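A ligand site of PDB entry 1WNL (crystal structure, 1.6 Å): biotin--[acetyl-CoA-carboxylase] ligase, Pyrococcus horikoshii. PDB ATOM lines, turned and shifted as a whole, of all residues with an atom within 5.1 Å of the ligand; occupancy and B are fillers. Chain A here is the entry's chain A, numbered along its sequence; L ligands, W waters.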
ATOM      1  N   GLY A  47     -25.231  -5.261  31.832  1.00  0.00           N
ATOM      2  CA  GLY A  47     -25.581  -6.599  32.289  1.00  0.00           C
ATOM      3  C   GLY A  47     -25.963  -6.723  33.756  1.00  0.00           C
ATOM      4  O   GLY A  47     -26.117  -5.724  34.462  1.00  0.00           O
ATOM      5  N   ARG A  48     -26.109  -7.974  34.191  1.00  0.00           N
ATOM      6  CA  ARG A  48     -26.499  -8.320  35.562  1.00  0.00           C
ATOM      7  C   ARG A  48     -25.629  -7.686  36.643  1.00  0.00           C
ATOM      8  O   ARG A  48     -26.107  -7.426  37.749  1.00  0.00           O
ATOM      9  CB  ARG A  48     -26.489  -9.846  35.718  1.00  0.00           C
ATOM     10  CG  ARG A  48     -26.961 -10.348  37.075  1.00  0.00           C
ATOM     11  CD  ARG A  48     -26.973 -11.866  37.120  1.00  0.00           C
ATOM     12  NE  ARG A  48     -25.640 -12.451  36.994  1.00  0.00           N
ATOM     13  CZ  ARG A  48     -24.790 -12.619  38.001  1.00  0.00           C
ATOM     14  NH1 ARG A  48     -25.134 -12.255  39.230  1.00  0.00           N
ATOM     15  NH2 ARG A  48     -23.593 -13.153  37.788  1.00  0.00           N
ATOM     16  N   LEU A  49     -24.368  -7.445  36.334  1.00  0.00           N
ATOM     17  CA  LEU A  49     -23.463  -6.839  37.293  1.00  0.00           C
ATOM     18  C   LEU A  49     -23.167  -5.384  36.948  1.00  0.00           C
ATOM     19  O   LEU A  49     -22.072  -4.873  37.211  1.00  0.00           O
ATOM     20  CB  LEU A  49     -22.156  -7.646  37.379  1.00  0.00           C
ATOM     21  CG  LEU A  49     -22.175  -8.933  38.233  1.00  0.00           C
ATOM     22  CD1 LEU A  49     -21.392  -8.680  39.504  1.00  0.00           C
ATOM     23  CD2 LEU A  49     -23.598  -9.365  38.549  1.00  0.00           C
ATOM     24  N   ASN A  50     -24.159  -4.730  36.367  1.00  0.00           N
ATOM     25  CA  ASN A  50     -24.071  -3.320  35.969  1.00  0.00           C
ATOM     26  C   ASN A  50     -22.843  -2.968  35.136  1.00  0.00           C
ATOM     27  O   ASN A  50     -22.374  -1.833  35.164  1.00  0.00           O
ATOM     28  CB  ASN A  50     -24.135  -2.429  37.210  1.00  0.00           C
ATOM     29  CG  ASN A  50     -24.460  -0.986  36.876  1.00  0.00           C
ATOM     30  OD1 ASN A  50     -25.336  -0.724  36.052  1.00  0.00           O
ATOM     31  ND2 ASN A  50     -23.773  -0.053  37.516  1.00  0.00           N
ATOM     32  N   ARG A  51     -22.340  -3.940  34.389  1.00  0.00           N
ATOM     33  CA  ARG A  51     -21.185  -3.716  33.536  1.00  0.00           C
ATOM     34  C   ARG A  51     -21.689  -3.465  32.114  1.00  0.00           C
ATOM     35  O   ARG A  51     -22.577  -4.178  31.631  1.00  0.00           O
ATOM     36  CB  ARG A  51     -20.246  -4.929  33.605  1.00  0.00           C
ATOM     37  CG  ARG A  51     -19.667  -5.103  35.009  1.00  0.00           C
ATOM     38  CD  ARG A  51     -18.904  -6.402  35.200  1.00  0.00           C
ATOM     39  NE  ARG A  51     -18.469  -6.538  36.594  1.00  0.00           N
ATOM     40  CZ  ARG A  51     -17.842  -7.592  37.091  1.00  0.00           C
ATOM     41  NH1 ARG A  51     -17.552  -8.626  36.332  1.00  0.00           N
ATOM     42  NH2 ARG A  51     -17.498  -7.610  38.378  1.00  0.00           N
ATOM     43  N   LYS A  52     -21.126  -2.459  31.452  1.00  0.00           N
ATOM     44  CA  LYS A  52     -21.554  -2.103  30.108  1.00  0.00           C
ATOM     45  C   LYS A  52     -21.829  -3.282  29.186  1.00  0.00           C
ATOM     46  O   LYS A  52     -21.061  -4.251  29.138  1.00  0.00           O
ATOM     47  CB  LYS A  52     -20.532  -1.174  29.441  1.00  0.00           C
ATOM     48  CG  LYS A  52     -20.893  -0.824  28.002  1.00  0.00           C
ATOM     49  CD  LYS A  52     -20.119   0.381  27.482  1.00  0.00           C
ATOM     50  CE  LYS A  52     -20.431   0.617  26.001  1.00  0.00           C
ATOM     51  NZ  LYS A  52     -21.906   0.697  25.742  1.00  0.00           N
ATOM     52  N   TRP A  53     -22.931  -3.190  28.458  1.00  0.00           N
ATOM     53  CA  TRP A  53     -23.334  -4.212  27.521  1.00  0.00           C
ATOM     54  C   TRP A  53     -23.391  -3.603  26.128  1.00  0.00           C
ATOM     55  O   TRP A  53     -23.965  -2.528  25.940  1.00  0.00           O
ATOM     56  CB  TRP A  53     -24.715  -4.767  27.919  1.00  0.00           C
ATOM     57  CG  TRP A  53     -25.203  -5.873  27.036  1.00  0.00           C
ATOM     58  CD1 TRP A  53     -25.826  -5.754  25.834  1.00  0.00           C
ATOM     59  CD2 TRP A  53     -25.038  -7.268  27.270  1.00  0.00           C
ATOM     60  NE1 TRP A  53     -26.062  -6.992  25.292  1.00  0.00           N
ATOM     61  CE2 TRP A  53     -25.592  -7.948  26.160  1.00  0.00           C
ATOM     62  CE3 TRP A  53     -24.482  -8.030  28.307  1.00  0.00           C
ATOM     63  CZ2 TRP A  53     -25.599  -9.342  26.050  1.00  0.00           C
ATOM     64  CZ3 TRP A  53     -24.489  -9.418  28.209  1.00  0.00           C
ATOM     65  CH2 TRP A  53     -25.041 -10.058  27.088  1.00  0.00           C
ATOM     66  N   GLU A  54     -22.768  -4.269  25.155  1.00  0.00           N
ATOM     67  CA  GLU A  54     -22.757  -3.781  23.777  1.00  0.00           C
ATOM     68  C   GLU A  54     -24.051  -4.231  23.087  1.00  0.00           C
ATOM     69  O   GLU A  54     -24.317  -5.431  22.993  1.00  0.00           O
ATOM     70  CB  GLU A  54     -21.553  -4.331  23.020  1.00  0.00           C
ATOM     71  CG  GLU A  54     -20.206  -3.874  23.546  1.00  0.00           C
ATOM     72  CD  GLU A  54     -20.045  -2.356  23.509  1.00  0.00           C
ATOM     73  OE1 GLU A  54     -20.308  -1.763  22.450  1.00  0.00           O
ATOM     74  OE2 GLU A  54     -19.646  -1.783  24.537  1.00  0.00           O
ATOM     75  N   TRP A  61     -32.520  -7.116  21.522  1.00  0.00           N
ATOM     76  CA  TRP A  61     -32.452  -6.409  22.789  1.00  0.00           C
ATOM     77  C   TRP A  61     -33.876  -6.114  23.233  1.00  0.00           C
ATOM     78  O   TRP A  61     -34.555  -5.278  22.648  1.00  0.00           O
ATOM     79  CB  TRP A  61     -31.691  -5.092  22.609  1.00  0.00           C
ATOM     80  CG  TRP A  61     -30.526  -5.186  21.658  1.00  0.00           C
ATOM     81  CD1 TRP A  61     -30.339  -4.475  20.499  1.00  0.00           C
ATOM     82  CD2 TRP A  61     -29.388  -6.049  21.773  1.00  0.00           C
ATOM     83  NE1 TRP A  61     -29.163  -4.839  19.898  1.00  0.00           N
ATOM     84  CE2 TRP A  61     -28.554  -5.794  20.656  1.00  0.00           C
ATOM     85  CE3 TRP A  61     -28.986  -7.011  22.711  1.00  0.00           C
ATOM     86  CZ2 TRP A  61     -27.343  -6.478  20.460  1.00  0.00           C
ATOM     87  CZ3 TRP A  61     -27.781  -7.684  22.510  1.00  0.00           C
ATOM     88  CH2 TRP A  61     -26.969  -7.409  21.385  1.00  0.00           C
ATOM     89  N   LYS A 100     -25.006 -20.647  31.998  1.00  0.00           N
ATOM     90  CA  LYS A 100     -23.923 -20.390  32.927  1.00  0.00           C
ATOM     91  C   LYS A 100     -24.641 -19.704  34.078  1.00  0.00           C
ATOM     92  O   LYS A 100     -25.180 -18.611  33.926  1.00  0.00           O
ATOM     93  CB  LYS A 100     -22.887 -19.444  32.337  1.00  0.00           C
ATOM     94  CG  LYS A 100     -21.914 -18.894  33.375  1.00  0.00           C
ATOM     95  CD  LYS A 100     -20.964 -17.866  32.765  1.00  0.00           C
ATOM     96  CE  LYS A 100     -20.068 -17.251  33.831  1.00  0.00           C
ATOM     97  NZ  LYS A 100     -19.177 -16.198  33.252  1.00  0.00           N
ATOM     98  N   ASP A 104     -26.650 -16.329  32.410  1.00  0.00           N
ATOM     99  CA  ASP A 104     -26.017 -16.272  31.102  1.00  0.00           C
ATOM    100  C   ASP A 104     -26.203 -17.510  30.249  1.00  0.00           C
ATOM    101  O   ASP A 104     -26.439 -18.609  30.765  1.00  0.00           O
ATOM    102  CB  ASP A 104     -24.522 -15.996  31.258  1.00  0.00           C
ATOM    103  CG  ASP A 104     -24.234 -14.697  31.965  1.00  0.00           C
ATOM    104  OD1 ASP A 104     -24.872 -13.678  31.618  1.00  0.00           O
ATOM    105  OD2 ASP A 104     -23.372 -14.694  32.873  1.00  0.00           O
ATOM    106  N   LYS A 111     -20.159 -16.289  25.595  1.00  0.00           N
ATOM    107  CA  LYS A 111     -21.473 -15.699  25.882  1.00  0.00           C
ATOM    108  C   LYS A 111     -22.254 -15.265  24.648  1.00  0.00           C
ATOM    109  O   LYS A 111     -21.779 -14.440  23.866  1.00  0.00           O
ATOM    110  CB  LYS A 111     -21.340 -14.527  26.849  1.00  0.00           C
ATOM    111  CG  LYS A 111     -22.686 -14.036  27.398  1.00  0.00           C
ATOM    112  CD  LYS A 111     -22.570 -12.745  28.206  1.00  0.00           C
ATOM    113  CE  LYS A 111     -21.740 -12.914  29.466  1.00  0.00           C
ATOM    114  NZ  LYS A 111     -21.752 -11.674  30.298  1.00  0.00           N
ATOM    115  N   ASN A 131     -27.238 -12.064  21.123  1.00  0.00           N
ATOM    116  CA  ASN A 131     -26.472 -11.721  19.936  1.00  0.00           C
ATOM    117  C   ASN A 131     -26.965 -12.573  18.773  1.00  0.00           C
ATOM    118  O   ASN A 131     -26.897 -13.809  18.825  1.00  0.00           O
ATOM    119  CB  ASN A 131     -24.977 -11.971  20.158  1.00  0.00           C
ATOM    120  CG  ASN A 131     -24.401 -11.120  21.254  1.00  0.00           C
ATOM    121  OD1 ASN A 131     -24.623  -9.908  21.301  1.00  0.00           O
ATOM    122  ND2 ASN A 131     -23.640 -11.745  22.149  1.00  0.00           N
ATOM    123  N   ASN A 134     -25.356  -9.233  15.013  1.00  0.00           N
ATOM    124  CA  ASN A 134     -24.466  -8.145  15.362  1.00  0.00           C
ATOM    125  C   ASN A 134     -23.033  -8.552  15.640  1.00  0.00           C
ATOM    126  O   ASN A 134     -22.736  -9.729  15.886  1.00  0.00           O
ATOM    127  CB  ASN A 134     -24.991  -7.429  16.611  1.00  0.00           C
ATOM    128  CG  ASN A 134     -25.230  -8.376  17.777  1.00  0.00           C
ATOM    129  OD1 ASN A 134     -26.112  -9.247  17.724  1.00  0.00           O
ATOM    130  ND2 ASN A 134     -24.445  -8.210  18.831  1.00  0.00           N
ATOM    131  N   VAL A 136     -19.857  -8.709  18.000  1.00  0.00           N
ATOM    132  CA  VAL A 136     -19.829  -8.915  19.436  1.00  0.00           C
ATOM    133  C   VAL A 136     -18.450  -8.646  20.027  1.00  0.00           C
ATOM    134  O   VAL A 136     -17.452  -8.597  19.307  1.00  0.00           O
ATOM    135  CB  VAL A 136     -20.248 -10.360  19.799  1.00  0.00           C
ATOM    136  CG1 VAL A 136     -21.612 -10.667  19.202  1.00  0.00           C
ATOM    137  CG2 VAL A 136     -19.214 -11.341  19.261  1.00  0.00           C
ATOM    138  N   PRO A 137     -18.375  -8.454  21.361  1.00  0.00           N
ATOM    139  CA  PRO A 137     -17.072  -8.191  21.992  1.00  0.00           C
ATOM    140  C   PRO A 137     -16.209  -9.439  21.845  1.00  0.00           C
ATOM    141  O   PRO A 137     -16.731 -10.555  21.732  1.00  0.00           O
ATOM    142  CB  PRO A 137     -17.444  -7.932  23.446  1.00  0.00           C
ATOM    143  CG  PRO A 137     -18.847  -7.419  23.366  1.00  0.00           C
ATOM    144  CD  PRO A 137     -19.461  -8.322  22.337  1.00  0.00           C
ATOM    145  N   ALA A 140     -17.045 -13.253  22.965  1.00  0.00           N
ATOM    146  CA  ALA A 140     -18.468 -13.562  22.938  1.00  0.00           C
ATOM    147  C   ALA A 140     -18.794 -14.209  21.603  1.00  0.00           C
ATOM    148  O   ALA A 140     -17.911 -14.408  20.766  1.00  0.00           O
ATOM    149  CB  ALA A 140     -19.286 -12.292  23.118  1.00  0.00           C
ATOM    150  N   SER A 231     -20.043 -13.103  40.821  1.00  0.00           N
ATOM    151  CA  SER A 231     -19.657 -13.442  39.459  1.00  0.00           C
ATOM    152  C   SER A 231     -19.094 -14.854  39.473  1.00  0.00           C
ATOM    153  O   SER A 231     -18.490 -15.278  40.446  1.00  0.00           O
ATOM    154  CB  SER A 231     -18.707 -12.541  38.644  1.00  0.00           C
ATOM    155  OG  SER A 231     -19.364 -11.289  38.855  1.00  0.00           O
ATOM    156  N   ARG A 233     -16.689 -17.628  37.418  1.00  0.00           N
ATOM    157  CA  ARG A 233     -15.685 -17.786  36.389  1.00  0.00           C
ATOM    158  C   ARG A 233     -15.310 -19.246  36.296  1.00  0.00           C
ATOM    159  O   ARG A 233     -15.122 -19.901  37.311  1.00  0.00           O
ATOM    160  CB  ARG A 233     -14.444 -16.942  36.726  1.00  0.00           C
ATOM    161  CG  ARG A 233     -14.675 -15.453  36.647  1.00  0.00           C
ATOM    162  CD  ARG A 233     -15.193 -15.067  35.271  1.00  0.00           C
ATOM    163  NE  ARG A 233     -15.609 -13.671  35.272  1.00  0.00           N
ATOM    164  CZ  ARG A 233     -16.337 -13.110  34.311  1.00  0.00           C
ATOM    165  NH1 ARG A 233     -16.733 -13.832  33.260  1.00  0.00           N
ATOM    166  NH2 ARG A 233     -16.678 -11.831  34.403  1.00  0.00           N
HETATM  167  P1  LIG L   1     -20.183 -10.625  34.017  1.00  0.00           P
HETATM  168  O1  LIG L   1     -19.010 -10.023  34.711  1.00  0.00           O
HETATM  169  O2  LIG L   1     -19.813 -11.531  32.885  1.00  0.00           O
HETATM  170  O3  LIG L   1     -21.195 -11.319  35.019  1.00  0.00           O
HETATM  171  P2  LIG L   1     -22.380  -8.819  33.366  1.00  0.00           P
HETATM  172  O4  LIG L   1     -23.343  -9.928  33.755  1.00  0.00           O
HETATM  173  O5  LIG L   1     -22.433  -7.577  34.215  1.00  0.00           O
HETATM  174  O6  LIG L   1     -20.914  -9.412  33.307  1.00  0.00           O
HETATM  175  O7  LIG L   1     -22.671  -8.587  31.830  1.00  0.00           O
HETATM  176  C1  LIG L   1     -21.901  -7.586  31.095  1.00  0.00           C
HETATM  177  C2  LIG L   1     -20.549  -8.115  30.587  1.00  0.00           C
HETATM  178  O8  LIG L   1     -20.816  -8.943  29.430  1.00  0.00           O
HETATM  179  C3  LIG L   1     -19.563  -7.053  30.085  1.00  0.00           C
HETATM  180  O9  LIG L   1     -18.709  -6.674  31.197  1.00  0.00           O
HETATM  181  C4  LIG L   1     -18.859  -7.752  28.903  1.00  0.00           C
HETATM  182  O10 LIG L   1     -17.652  -8.432  29.280  1.00  0.00           O
HETATM  183  C5  LIG L   1     -19.877  -8.777  28.390  1.00  0.00           C
HETATM  184  N1  LIG L   1     -20.668  -8.301  27.183  1.00  0.00           N
HETATM  185  C6  LIG L   1     -20.985  -7.018  26.831  1.00  0.00           C
HETATM  186  N2  LIG L   1     -21.714  -6.936  25.717  1.00  0.00           N
HETATM  187  C7  LIG L   1     -21.875  -8.227  25.329  1.00  0.00           C
HETATM  188  C8  LIG L   1     -22.578  -8.803  24.210  1.00  0.00           C
HETATM  189  N3  LIG L   1     -23.219  -8.155  23.296  1.00  0.00           N
HETATM  190  N4  LIG L   1     -22.515 -10.190  24.163  1.00  0.00           N
HETATM  191  C9  LIG L   1     -21.844 -10.966  25.105  1.00  0.00           C
HETATM  192  N5  LIG L   1     -21.194 -10.444  26.151  1.00  0.00           N
HETATM  193  C10 LIG L   1     -21.237  -9.085  26.227  1.00  0.00           C
HETATM  194  O   HOH W   1     -17.078  -8.468  33.017  1.00  0.00           O
HETATM  195  O   HOH W   2     -18.649 -11.563  30.030  1.00  0.00           O
HETATM  196  O   HOH W   3     -23.483 -12.605  34.455  1.00  0.00           O
HETATM  197  O   HOH W   4     -20.832 -14.107  36.278  1.00  0.00           O
HETATM  198  O   HOH W   5     -18.643 -11.983  26.708  1.00  0.00           O
HETATM  199  O   HOH W   6     -20.680 -14.190  32.462  1.00  0.00           O
HETATM  200  O   HOH W   7     -16.106  -7.818  26.633  1.00  0.00           O
HETATM  201  O   HOH W   8     -24.260 -11.139  31.359  1.00  0.00           O
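Water W3 lies within hydrogen-bond range of OD2 of Asp 104 (2.6 Å), O3 of the ligand (2.7 Å) and NE of Arg 48 (3.3 Å). Water W6 lies within hydrogen-bond range of the side-chain amino group of Lys 100, the side-chain carboxylate of Asp 104, an oxygen (O2) of the ligand and the side-chain amino group of Lys 111. Water W8 lies within hydrogen-bond range of OD1 of Asp 104 (2.6 Å), NZ of Lys 111 (2.8 Å) and O4 of the ligand (2.8 Å). Water W1 lies within hydrogen-bond range of an oxygen (O1) of the ligand and the guanidinium group of Arg 51. Water W4 bridges O3 of the ligand and NH2 of Arg 48. Water W2 bridges O2 of the ligand (3.1 Å) and NZ of Lys 111 (3.1 Å).
The side-chain amide oxygen of Asn 131 is in hydrogen-bond range of the side-chain amide nitrogen of Asn 134, 3.0 Å away. The side-chain amino group of Lys 52 lies within salt-bridge range of the side-chain carboxylate of Glu 54, 3.6 Å away. The side-chain amino group (NZ) of Lys 111 is in salt-bridge range of the side-chain carboxylate (OD1) of Asp 104 (3.9 Å).
NH1 of Arg 51 lies within salt-bridge range of O1 of the ligand, 2.6 Å away. The side-chain amide nitrogen (ND2) of Asn 131 is in hydrogen-bond range of a nitrogen (N4) of the ligand (2.8 Å). O5 of the ligand sits at hydrogen-bond distance from N of Leu 49, 2.9 Å away. N of Glu 54 is in hydrogen-bond range of N2 of the ligand (2.9 Å). N3 of the ligand is in hydrogen-bond range of O of Glu 54, at 3.0 Å. An oxygen (O1) of the ligand lies within salt-bridge range of the guanidinium group of Arg 233 (3.0 Å). The side-chain amino group (NZ) of Lys 111 lies within salt-bridge range of an oxygen (O2) of the ligand. An oxygen (O4) of the ligand lies within hydrogen-bond range of the backbone NH (N) of Arg 48, 3.4 Å away.
CA of Gly 47 touches O7 of the ligand, 3.6 Å away. N of Asn 50 touches O5 of the ligand, at 3.96 Å. Lys 52 touches the ligand (O to C3, 3.3 Å). Trp 53 touches the ligand. Pro 137 touches the ligand. CB of Ala 140 touches C9 of the ligand, 3.5 Å away. Hydrophobic or aromatic side chains that line the ligand: Leu 49, Trp 53, Pro 137 and Ala 140. Of the 19 residues printed, 13 come within 4 Å of the ligand.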
